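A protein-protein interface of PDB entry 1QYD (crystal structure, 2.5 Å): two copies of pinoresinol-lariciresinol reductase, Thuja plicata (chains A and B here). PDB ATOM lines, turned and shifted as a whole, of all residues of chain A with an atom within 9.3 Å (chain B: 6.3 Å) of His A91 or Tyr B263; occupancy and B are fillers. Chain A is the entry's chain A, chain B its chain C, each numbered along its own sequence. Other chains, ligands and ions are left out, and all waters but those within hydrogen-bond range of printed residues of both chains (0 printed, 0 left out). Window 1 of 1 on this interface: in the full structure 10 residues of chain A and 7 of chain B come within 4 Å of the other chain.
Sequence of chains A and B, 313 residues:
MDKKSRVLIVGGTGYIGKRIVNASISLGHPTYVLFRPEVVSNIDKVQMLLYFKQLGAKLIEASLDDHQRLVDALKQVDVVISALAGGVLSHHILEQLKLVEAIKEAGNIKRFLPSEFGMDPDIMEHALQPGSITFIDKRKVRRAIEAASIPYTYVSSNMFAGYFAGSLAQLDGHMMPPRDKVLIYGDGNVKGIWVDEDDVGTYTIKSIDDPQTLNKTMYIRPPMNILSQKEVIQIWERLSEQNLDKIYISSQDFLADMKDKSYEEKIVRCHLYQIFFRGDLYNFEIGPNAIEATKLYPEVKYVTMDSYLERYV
Hydrophobic or aromatic side chains of chain A within 4 Å of the printed part of chain B: His A91 and Leu A94. Of the 10 printed residues of chain B, 3 touch a printed residue of chain A.
Of the printed residues of chain B, Asp A65 touches Lys B266 (3.4 Å). His A91 touches just these residues of chain B: Tyr B263 (3.2 Å) and Glu B264 (3.1 Å). Of the printed residues of chain B, Leu A94 touches Tyr B263 (3.7 Å). Of the printed residues of chain B, Glu A95 touches Tyr B263 (3.4 Å) and Lys B266 (3.5 Å). Of the printed residues of chain B, Lys A98 touches Lys B266. Ser B262 touches none of the printed residues of chain A. Of chain A, only His A91 (3.2 Å), Leu A94 (3.7 Å) and Glu A95 (3.4 Å) come within 4 Å of Tyr B263. Glu B264 touches one residue of chain A. Of the printed residues of chain A, Lys B266 touches Asp A65, Glu A95 and Lys A98. The nearest printed residue of chain A that does not touch Tyr B263 is Ser A90 (5.1 Å).
NZ of Lys B266 is in salt-bridge range of OD2 of Asp A65, at 3.999 Å. NE2 of His A91 sits close to OE1 of Glu B264 (3.3 Å). The side-chain amino group (NZ) of Lys B266 is in salt-bridge range of the side-chain carboxylate (OE2) of Glu A95, 3.5 Å away.
OD2 of Asp A65 lies within salt-bridge range of NZ of Lys A98 (3.9 Å). OE2 of Glu A95 lies within salt-bridge range of NZ of Lys A98 (3.1 Å).
O of His A91 touches CE2 of Tyr B263 (3.2 Å). Tyr B263 touches Leu A94. OE2 of Glu A95 touches CE2 of Tyr B263, at 3.4 Å. Lys A98 touches Lys B266.
1 position is printed for both chains. Of the 7 pairs that touch across the chains among the printed residues, none has its exchanged pair printed and touching as well.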
ATOM      1  N   LEU A  64      24.957  -8.463 -19.163  1.00  0.00           N
ATOM      2  CA  LEU A  64      25.792  -8.962 -20.246  1.00  0.00           C
ATOM      3  C   LEU A  64      27.269  -9.061 -19.937  1.00  0.00           C
ATOM      4  O   LEU A  64      28.025  -9.772 -20.615  1.00  0.00           O
ATOM      5  CB  LEU A  64      25.619  -8.081 -21.434  1.00  0.00           C
ATOM      6  CG  LEU A  64      24.337  -8.306 -22.151  1.00  0.00           C
ATOM      7  CD1 LEU A  64      23.919  -7.000 -22.786  1.00  0.00           C
ATOM      8  CD2 LEU A  64      24.503  -9.442 -23.122  1.00  0.00           C
ATOM      9  N   ASP A  65      27.635  -8.292 -18.900  1.00  0.00           N
ATOM     10  CA  ASP A  65      28.998  -8.223 -18.406  1.00  0.00           C
ATOM     11  C   ASP A  65      29.430  -9.425 -17.597  1.00  0.00           C
ATOM     12  O   ASP A  65      30.622  -9.735 -17.539  1.00  0.00           O
ATOM     13  CB  ASP A  65      29.158  -6.970 -17.565  1.00  0.00           C
ATOM     14  CG  ASP A  65      29.457  -5.725 -18.380  1.00  0.00           C
ATOM     15  OD1 ASP A  65      30.358  -4.983 -17.973  1.00  0.00           O
ATOM     16  OD2 ASP A  65      28.791  -5.510 -19.400  1.00  0.00           O
ATOM     17  N   LEU A  84      18.466  -6.315 -29.064  1.00  0.00           N
ATOM     18  CA  LEU A  84      19.177  -5.258 -28.354  1.00  0.00           C
ATOM     19  C   LEU A  84      19.383  -3.992 -29.157  1.00  0.00           C
ATOM     20  O   LEU A  84      20.258  -3.972 -30.023  1.00  0.00           O
ATOM     21  CB  LEU A  84      20.565  -5.792 -27.879  1.00  0.00           C
ATOM     22  CG  LEU A  84      20.581  -6.463 -26.484  1.00  0.00           C
ATOM     23  CD1 LEU A  84      21.885  -7.175 -26.133  1.00  0.00           C
ATOM     24  CD2 LEU A  84      20.303  -5.334 -25.508  1.00  0.00           C
ATOM     25  N   ALA A  85      18.603  -2.930 -28.888  1.00  0.00           N
ATOM     26  CA  ALA A  85      18.741  -1.639 -29.586  1.00  0.00           C
ATOM     27  C   ALA A  85      18.093  -0.418 -28.925  1.00  0.00           C
ATOM     28  O   ALA A  85      17.077  -0.510 -28.223  1.00  0.00           O
ATOM     29  CB  ALA A  85      18.153  -1.705 -30.994  1.00  0.00           C
ATOM     30  N   GLY A  86      18.647   0.771 -29.195  1.00  0.00           N
ATOM     31  CA  GLY A  86      18.140   1.987 -28.570  1.00  0.00           C
ATOM     32  C   GLY A  86      18.480   3.247 -29.340  1.00  0.00           C
ATOM     33  O   GLY A  86      18.108   3.357 -30.513  1.00  0.00           O
ATOM     34  N   GLY A  87      19.220   4.171 -28.696  1.00  0.00           N
ATOM     35  CA  GLY A  87      19.557   5.480 -29.249  1.00  0.00           C
ATOM     36  C   GLY A  87      20.321   5.471 -30.562  1.00  0.00           C
ATOM     37  O   GLY A  87      19.869   4.990 -31.604  1.00  0.00           O
ATOM     38  N   VAL A  88      21.528   6.028 -30.467  1.00  0.00           N
ATOM     39  CA  VAL A  88      22.493   6.161 -31.559  1.00  0.00           C
ATOM     40  C   VAL A  88      22.718   4.866 -32.381  1.00  0.00           C
ATOM     41  O   VAL A  88      23.276   4.907 -33.481  1.00  0.00           O
ATOM     42  CB  VAL A  88      23.821   6.680 -30.913  1.00  0.00           C
ATOM     43  CG1 VAL A  88      24.806   7.027 -32.013  1.00  0.00           C
ATOM     44  CG2 VAL A  88      23.569   7.893 -30.009  1.00  0.00           C
ATOM     45  N   LEU A  89      22.207   3.721 -31.859  1.00  0.00           N
ATOM     46  CA  LEU A  89      22.309   2.342 -32.351  1.00  0.00           C
ATOM     47  C   LEU A  89      23.760   1.857 -32.397  1.00  0.00           C
ATOM     48  O   LEU A  89      24.220   1.108 -33.271  1.00  0.00           O
ATOM     49  CB  LEU A  89      21.658   2.247 -33.738  1.00  0.00           C
ATOM     50  CG  LEU A  89      20.137   2.313 -33.788  1.00  0.00           C
ATOM     51  CD1 LEU A  89      19.684   2.461 -35.235  1.00  0.00           C
ATOM     52  CD2 LEU A  89      19.554   1.064 -33.126  1.00  0.00           C
ATOM     53  N   SER A  90      24.451   2.305 -31.339  1.00  0.00           N
ATOM     54  CA  SER A  90      25.868   2.100 -31.199  1.00  0.00           C
ATOM     55  C   SER A  90      26.278   1.484 -29.882  1.00  0.00           C
ATOM     56  O   SER A  90      26.865   0.401 -29.885  1.00  0.00           O
ATOM     57  CB  SER A  90      26.572   3.448 -31.422  1.00  0.00           C
ATOM     58  OG  SER A  90      27.815   3.274 -32.099  1.00  0.00           O
ATOM     59  N   HIS A  91      25.929   2.168 -28.774  1.00  0.00           N
ATOM     60  CA  HIS A  91      26.205   1.834 -27.370  1.00  0.00           C
ATOM     61  C   HIS A  91      25.672   0.481 -26.889  1.00  0.00           C
ATOM     62  O   HIS A  91      26.193  -0.132 -25.957  1.00  0.00           O
ATOM     63  CB  HIS A  91      25.639   3.054 -26.625  1.00  0.00           C
ATOM     64  CG  HIS A  91      25.431   3.153 -25.113  1.00  0.00           C
ATOM     65  ND1 HIS A  91      24.652   2.442 -24.293  1.00  0.00           N
ATOM     66  CD2 HIS A  91      26.015   4.145 -24.362  1.00  0.00           C
ATOM     67  CE1 HIS A  91      24.756   2.983 -23.097  1.00  0.00           C
ATOM     68  NE2 HIS A  91      25.576   4.008 -23.140  1.00  0.00           N
ATOM     69  N   HIS A  92      24.703  -0.055 -27.620  1.00  0.00           N
ATOM     70  CA  HIS A  92      23.941  -1.230 -27.237  1.00  0.00           C
ATOM     71  C   HIS A  92      23.914  -2.318 -28.290  1.00  0.00           C
ATOM     72  O   HIS A  92      23.522  -3.451 -28.006  1.00  0.00           O
ATOM     73  CB  HIS A  92      22.512  -0.774 -26.885  1.00  0.00           C
ATOM     74  CG  HIS A  92      22.230   0.629 -27.412  1.00  0.00           C
ATOM     75  ND1 HIS A  92      22.302   1.009 -28.682  1.00  0.00           N
ATOM     76  CD2 HIS A  92      22.002   1.726 -26.631  1.00  0.00           C
ATOM     77  CE1 HIS A  92      22.144   2.304 -28.676  1.00  0.00           C
ATOM     78  NE2 HIS A  92      21.964   2.734 -27.453  1.00  0.00           N
ATOM     79  N   ILE A  93      24.297  -1.988 -29.523  1.00  0.00           N
ATOM     80  CA  ILE A  93      24.415  -2.969 -30.593  1.00  0.00           C
ATOM     81  C   ILE A  93      25.712  -3.755 -30.450  1.00  0.00           C
ATOM     82  O   ILE A  93      25.708  -4.964 -30.660  1.00  0.00           O
ATOM     83  CB  ILE A  93      24.331  -2.234 -31.972  1.00  0.00           C
ATOM     84  CG1 ILE A  93      22.834  -2.125 -32.258  1.00  0.00           C
ATOM     85  CG2 ILE A  93      25.055  -2.938 -33.133  1.00  0.00           C
ATOM     86  CD1 ILE A  93      22.468  -1.476 -33.614  1.00  0.00           C
ATOM     87  N   LEU A  94      26.811  -3.068 -30.100  1.00  0.00           N
ATOM     88  CA  LEU A  94      28.134  -3.636 -29.824  1.00  0.00           C
ATOM     89  C   LEU A  94      28.339  -4.371 -28.490  1.00  0.00           C
ATOM     90  O   LEU A  94      29.441  -4.801 -28.165  1.00  0.00           O
ATOM     91  CB  LEU A  94      29.128  -2.498 -29.945  1.00  0.00           C
ATOM     92  CG  LEU A  94      29.922  -2.240 -31.221  1.00  0.00           C
ATOM     93  CD1 LEU A  94      29.222  -2.696 -32.486  1.00  0.00           C
ATOM     94  CD2 LEU A  94      30.167  -0.774 -31.254  1.00  0.00           C
ATOM     95  N   GLU A  95      27.280  -4.478 -27.675  1.00  0.00           N
ATOM     96  CA  GLU A  95      27.215  -5.233 -26.418  1.00  0.00           C
ATOM     97  C   GLU A  95      27.051  -6.697 -26.736  1.00  0.00           C
ATOM     98  O   GLU A  95      27.437  -7.578 -25.987  1.00  0.00           O
ATOM     99  CB  GLU A  95      26.018  -4.812 -25.579  1.00  0.00           C
ATOM    100  CG  GLU A  95      26.208  -3.494 -24.841  1.00  0.00           C
ATOM    101  CD  GLU A  95      26.917  -3.562 -23.480  1.00  0.00           C
ATOM    102  OE1 GLU A  95      26.518  -4.367 -22.629  1.00  0.00           O
ATOM    103  OE2 GLU A  95      27.843  -2.772 -23.264  1.00  0.00           O
ATOM    104  N   GLN A  96      26.406  -6.940 -27.867  1.00  0.00           N
ATOM    105  CA  GLN A  96      26.195  -8.244 -28.458  1.00  0.00           C
ATOM    106  C   GLN A  96      27.487  -9.001 -28.733  1.00  0.00           C
ATOM    107  O   GLN A  96      27.400 -10.193 -29.017  1.00  0.00           O
ATOM    108  CB  GLN A  96      25.486  -8.097 -29.755  1.00  0.00           C
ATOM    109  CG  GLN A  96      24.176  -7.411 -29.611  1.00  0.00           C
ATOM    110  CD  GLN A  96      23.510  -7.373 -30.960  1.00  0.00           C
ATOM    111  OE1 GLN A  96      23.710  -6.464 -31.744  1.00  0.00           O
ATOM    112  NE2 GLN A  96      22.720  -8.374 -31.281  1.00  0.00           N
ATOM    113  N   LEU A  97      28.666  -8.338 -28.737  1.00  0.00           N
ATOM    114  CA  LEU A  97      29.973  -8.969 -28.942  1.00  0.00           C
ATOM    115  C   LEU A  97      30.318  -9.890 -27.778  1.00  0.00           C
ATOM    116  O   LEU A  97      30.682 -11.047 -27.986  1.00  0.00           O
ATOM    117  CB  LEU A  97      31.010  -7.859 -29.142  1.00  0.00           C
ATOM    118  CG  LEU A  97      30.916  -7.196 -30.558  1.00  0.00           C
ATOM    119  CD1 LEU A  97      31.700  -5.919 -30.626  1.00  0.00           C
ATOM    120  CD2 LEU A  97      31.520  -8.106 -31.609  1.00  0.00           C
ATOM    121  N   LYS A  98      30.069  -9.381 -26.559  1.00  0.00           N
ATOM    122  CA  LYS A  98      30.071 -10.095 -25.289  1.00  0.00           C
ATOM    123  C   LYS A  98      29.162 -11.304 -25.393  1.00  0.00           C
ATOM    124  O   LYS A  98      29.579 -12.399 -25.051  1.00  0.00           O
ATOM    125  CB  LYS A  98      29.513  -9.251 -24.151  1.00  0.00           C
ATOM    126  CG  LYS A  98      30.062  -7.842 -23.979  1.00  0.00           C
ATOM    127  CD  LYS A  98      29.559  -7.304 -22.660  1.00  0.00           C
ATOM    128  CE  LYS A  98      30.384  -6.096 -22.246  1.00  0.00           C
ATOM    129  NZ  LYS A  98      30.075  -4.924 -23.045  1.00  0.00           N
ATOM    130  N   ILE A 133      26.925   4.437 -39.316  1.00  0.00           N
ATOM    131  CA  ILE A 133      27.371   3.786 -38.070  1.00  0.00           C
ATOM    132  C   ILE A 133      26.576   2.548 -37.686  1.00  0.00           C
ATOM    133  O   ILE A 133      27.117   1.539 -37.257  1.00  0.00           O
ATOM    134  CB  ILE A 133      27.315   4.894 -36.983  1.00  0.00           C
ATOM    135  CG1 ILE A 133      28.755   5.163 -36.590  1.00  0.00           C
ATOM    136  CG2 ILE A 133      26.453   4.558 -35.765  1.00  0.00           C
ATOM    137  CD1 ILE A 133      29.454   4.137 -35.650  1.00  0.00           C
ATOM    138  N   THR A 134      25.264   2.598 -37.848  1.00  0.00           N
ATOM    139  CA  THR A 134      24.384   1.492 -37.537  1.00  0.00           C
ATOM    140  C   THR A 134      24.795   0.279 -38.352  1.00  0.00           C
ATOM    141  O   THR A 134      24.914  -0.831 -37.828  1.00  0.00           O
ATOM    142  CB  THR A 134      22.945   1.958 -37.863  1.00  0.00           C
ATOM    143  OG1 THR A 134      22.663   2.964 -36.898  1.00  0.00           O
ATOM    144  CG2 THR A 134      21.886   0.885 -37.803  1.00  0.00           C
ATOM    145  N   ASP A 137      28.295  -0.932 -37.176  1.00  0.00           N
ATOM    146  CA  ASP A 137      28.197  -1.640 -35.921  1.00  0.00           C
ATOM    147  C   ASP A 137      27.733  -3.056 -36.065  1.00  0.00           C
ATOM    148  O   ASP A 137      28.458  -3.971 -35.700  1.00  0.00           O
ATOM    149  CB  ASP A 137      27.253  -0.925 -35.008  1.00  0.00           C
ATOM    150  CG  ASP A 137      27.734   0.362 -34.339  1.00  0.00           C
ATOM    151  OD1 ASP A 137      28.870   0.852 -34.477  1.00  0.00           O
ATOM    152  OD2 ASP A 137      26.886   0.882 -33.644  1.00  0.00           O
ATOM    153  N   LYS A 140      30.296  -5.598 -37.545  1.00  0.00           N
ATOM    154  CA  LYS A 140      31.286  -6.063 -36.584  1.00  0.00           C
ATOM    155  C   LYS A 140      30.810  -7.284 -35.815  1.00  0.00           C
ATOM    156  O   LYS A 140      31.532  -8.267 -35.613  1.00  0.00           O
ATOM    157  CB  LYS A 140      31.600  -4.980 -35.580  1.00  0.00           C
ATOM    158  CG  LYS A 140      32.544  -4.003 -36.184  1.00  0.00           C
ATOM    159  CD  LYS A 140      33.162  -3.332 -34.978  1.00  0.00           C
ATOM    160  CE  LYS A 140      34.672  -3.212 -35.180  1.00  0.00           C
ATOM    161  NZ  LYS A 140      35.044  -2.296 -36.253  1.00  0.00           N
ATOM    162  N   VAL A 141      29.537  -7.166 -35.450  1.00  0.00           N
ATOM    163  CA  VAL A 141      28.760  -8.182 -34.785  1.00  0.00           C
ATOM    164  C   VAL A 141      28.540  -9.358 -35.732  1.00  0.00           C
ATOM    165  O   VAL A 141      28.678 -10.495 -35.273  1.00  0.00           O
ATOM    166  CB  VAL A 141      27.467  -7.470 -34.351  1.00  0.00           C
ATOM    167  CG1 VAL A 141      26.351  -8.429 -33.941  1.00  0.00           C
ATOM    168  CG2 VAL A 141      27.874  -6.538 -33.191  1.00  0.00           C
ATOM    169  N   PRO B 130      36.196  -1.467 -21.719  1.00  0.00           N
ATOM    170  CA  PRO B 130      36.067  -0.756 -22.980  1.00  0.00           C
ATOM    171  C   PRO B 130      36.986   0.414 -23.221  1.00  0.00           C
ATOM    172  O   PRO B 130      37.057   0.879 -24.349  1.00  0.00           O
ATOM    173  CB  PRO B 130      34.633  -0.340 -23.028  1.00  0.00           C
ATOM    174  CG  PRO B 130      34.010  -0.802 -21.730  1.00  0.00           C
ATOM    175  CD  PRO B 130      35.211  -0.874 -20.806  1.00  0.00           C
ATOM    176  N   ILE B 133      38.997   1.223 -26.458  1.00  0.00           N
ATOM    177  CA  ILE B 133      38.195   1.663 -27.587  1.00  0.00           C
ATOM    178  C   ILE B 133      38.145   3.175 -27.601  1.00  0.00           C
ATOM    179  O   ILE B 133      37.106   3.834 -27.618  1.00  0.00           O
ATOM    180  CB  ILE B 133      36.810   0.990 -27.426  1.00  0.00           C
ATOM    181  CG1 ILE B 133      36.995  -0.568 -27.231  1.00  0.00           C
ATOM    182  CG2 ILE B 133      35.942   1.382 -28.632  1.00  0.00           C
ATOM    183  CD1 ILE B 133      35.788  -1.461 -26.847  1.00  0.00           C
ATOM    184  N   LYS B 261      28.661  -0.492 -14.472  1.00  0.00           N
ATOM    185  CA  LYS B 261      28.344   0.845 -14.958  1.00  0.00           C
ATOM    186  C   LYS B 261      28.161   1.000 -16.471  1.00  0.00           C
ATOM    187  O   LYS B 261      28.373   0.076 -17.261  1.00  0.00           O
ATOM    188  CB  LYS B 261      29.431   1.791 -14.485  1.00  0.00           C
ATOM    189  CG  LYS B 261      29.295   2.288 -13.040  1.00  0.00           C
ATOM    190  CD  LYS B 261      29.115   1.172 -12.007  1.00  0.00           C
ATOM    191  CE  LYS B 261      29.198   1.620 -10.567  1.00  0.00           C
ATOM    192  NZ  LYS B 261      28.734   0.542  -9.704  1.00  0.00           N
ATOM    193  N   SER B 262      27.721   2.208 -16.867  1.00  0.00           N
ATOM    194  CA  SER B 262      27.432   2.647 -18.240  1.00  0.00           C
ATOM    195  C   SER B 262      28.654   2.814 -19.132  1.00  0.00           C
ATOM    196  O   SER B 262      29.666   3.291 -18.626  1.00  0.00           O
ATOM    197  CB  SER B 262      26.662   3.963 -18.142  1.00  0.00           C
ATOM    198  OG  SER B 262      27.102   4.851 -17.110  1.00  0.00           O
ATOM    199  N   TYR B 263      28.581   2.468 -20.434  1.00  0.00           N
ATOM    200  CA  TYR B 263      29.699   2.530 -21.370  1.00  0.00           C
ATOM    201  C   TYR B 263      30.699   3.658 -21.230  1.00  0.00           C
ATOM    202  O   TYR B 263      31.894   3.407 -21.347  1.00  0.00           O
ATOM    203  CB  TYR B 263      29.196   2.597 -22.768  1.00  0.00           C
ATOM    204  CG  TYR B 263      29.764   1.635 -23.803  1.00  0.00           C
ATOM    205  CD1 TYR B 263      30.973   1.831 -24.505  1.00  0.00           C
ATOM    206  CD2 TYR B 263      28.938   0.547 -24.128  1.00  0.00           C
ATOM    207  CE1 TYR B 263      31.330   0.936 -25.541  1.00  0.00           C
ATOM    208  CE2 TYR B 263      29.281  -0.345 -25.152  1.00  0.00           C
ATOM    209  CZ  TYR B 263      30.462  -0.149 -25.855  1.00  0.00           C
ATOM    210  OH  TYR B 263      30.689  -1.055 -26.876  1.00  0.00           O
ATOM    211  N   GLU B 264      30.293   4.907 -20.975  1.00  0.00           N
ATOM    212  CA  GLU B 264      31.247   6.013 -20.854  1.00  0.00           C
ATOM    213  C   GLU B 264      31.868   6.089 -19.466  1.00  0.00           C
ATOM    214  O   GLU B 264      32.804   6.868 -19.254  1.00  0.00           O
ATOM    215  CB  GLU B 264      30.622   7.391 -21.095  1.00  0.00           C
ATOM    216  CG  GLU B 264      29.711   7.524 -22.294  1.00  0.00           C
ATOM    217  CD  GLU B 264      28.328   6.868 -22.209  1.00  0.00           C
ATOM    218  OE1 GLU B 264      27.866   6.399 -23.250  1.00  0.00           O
ATOM    219  OE2 GLU B 264      27.715   6.838 -21.128  1.00  0.00           O
ATOM    220  N   GLU B 265      31.320   5.342 -18.493  1.00  0.00           N
ATOM    221  CA  GLU B 265      31.891   5.287 -17.157  1.00  0.00           C
ATOM    222  C   GLU B 265      32.878   4.120 -17.151  1.00  0.00           C
ATOM    223  O   GLU B 265      34.012   4.276 -16.694  1.00  0.00           O
ATOM    224  CB  GLU B 265      30.796   5.074 -16.121  1.00  0.00           C
ATOM    225  CG  GLU B 265      31.245   5.772 -14.829  1.00  0.00           C
ATOM    226  CD  GLU B 265      30.261   5.849 -13.651  1.00  0.00           C
ATOM    227  OE1 GLU B 265      30.660   6.331 -12.588  1.00  0.00           O
ATOM    228  OE2 GLU B 265      29.098   5.457 -13.778  1.00  0.00           O
ATOM    229  N   LYS B 266      32.516   2.947 -17.706  1.00  0.00           N
ATOM    230  CA  LYS B 266      33.476   1.866 -17.852  1.00  0.00           C
ATOM    231  C   LYS B 266      34.770   2.383 -18.517  1.00  0.00           C
ATOM    232  O   LYS B 266      35.836   2.143 -17.959  1.00  0.00           O
ATOM    233  CB  LYS B 266      32.875   0.730 -18.691  1.00  0.00           C
ATOM    234  CG  LYS B 266      31.682  -0.043 -18.100  1.00  0.00           C
ATOM    235  CD  LYS B 266      31.537  -1.469 -18.717  1.00  0.00           C
ATOM    236  CE  LYS B 266      30.102  -1.859 -19.165  1.00  0.00           C
ATOM    237  NZ  LYS B 266      29.979  -1.892 -20.622  1.00  0.00           N
ATOM    238  N   ILE B 267      34.740   3.205 -19.579  1.00  0.00           N
ATOM    239  CA  ILE B 267      35.939   3.772 -20.208  1.00  0.00           C
ATOM    240  C   ILE B 267      36.868   4.532 -19.244  1.00  0.00           C
ATOM    241  O   ILE B 267      38.062   4.226 -19.221  1.00  0.00           O
ATOM    242  CB  ILE B 267      35.469   4.703 -21.384  1.00  0.00           C
ATOM    243  CG1 ILE B 267      34.971   3.880 -22.556  1.00  0.00           C
ATOM    244  CG2 ILE B 267      36.595   5.576 -21.902  1.00  0.00           C
ATOM    245  CD1 ILE B 267      34.290   4.729 -23.667  1.00  0.00           C
ATOM    246  N   VAL B 268      36.363   5.476 -18.411  1.00  0.00           N
ATOM    247  CA  VAL B 268      37.201   6.306 -17.516  1.00  0.00           C
ATOM    248  C   VAL B 268      37.840   5.491 -16.417  1.00  0.00           C
ATOM    249  O   VAL B 268      38.978   5.707 -15.994  1.00  0.00           O
ATOM    250  CB  VAL B 268      36.364   7.524 -16.864  1.00  0.00           C
ATOM    251  CG1 VAL B 268      35.146   7.030 -16.146  1.00  0.00           C
ATOM    252  CG2 VAL B 268      37.176   8.275 -15.782  1.00  0.00           C
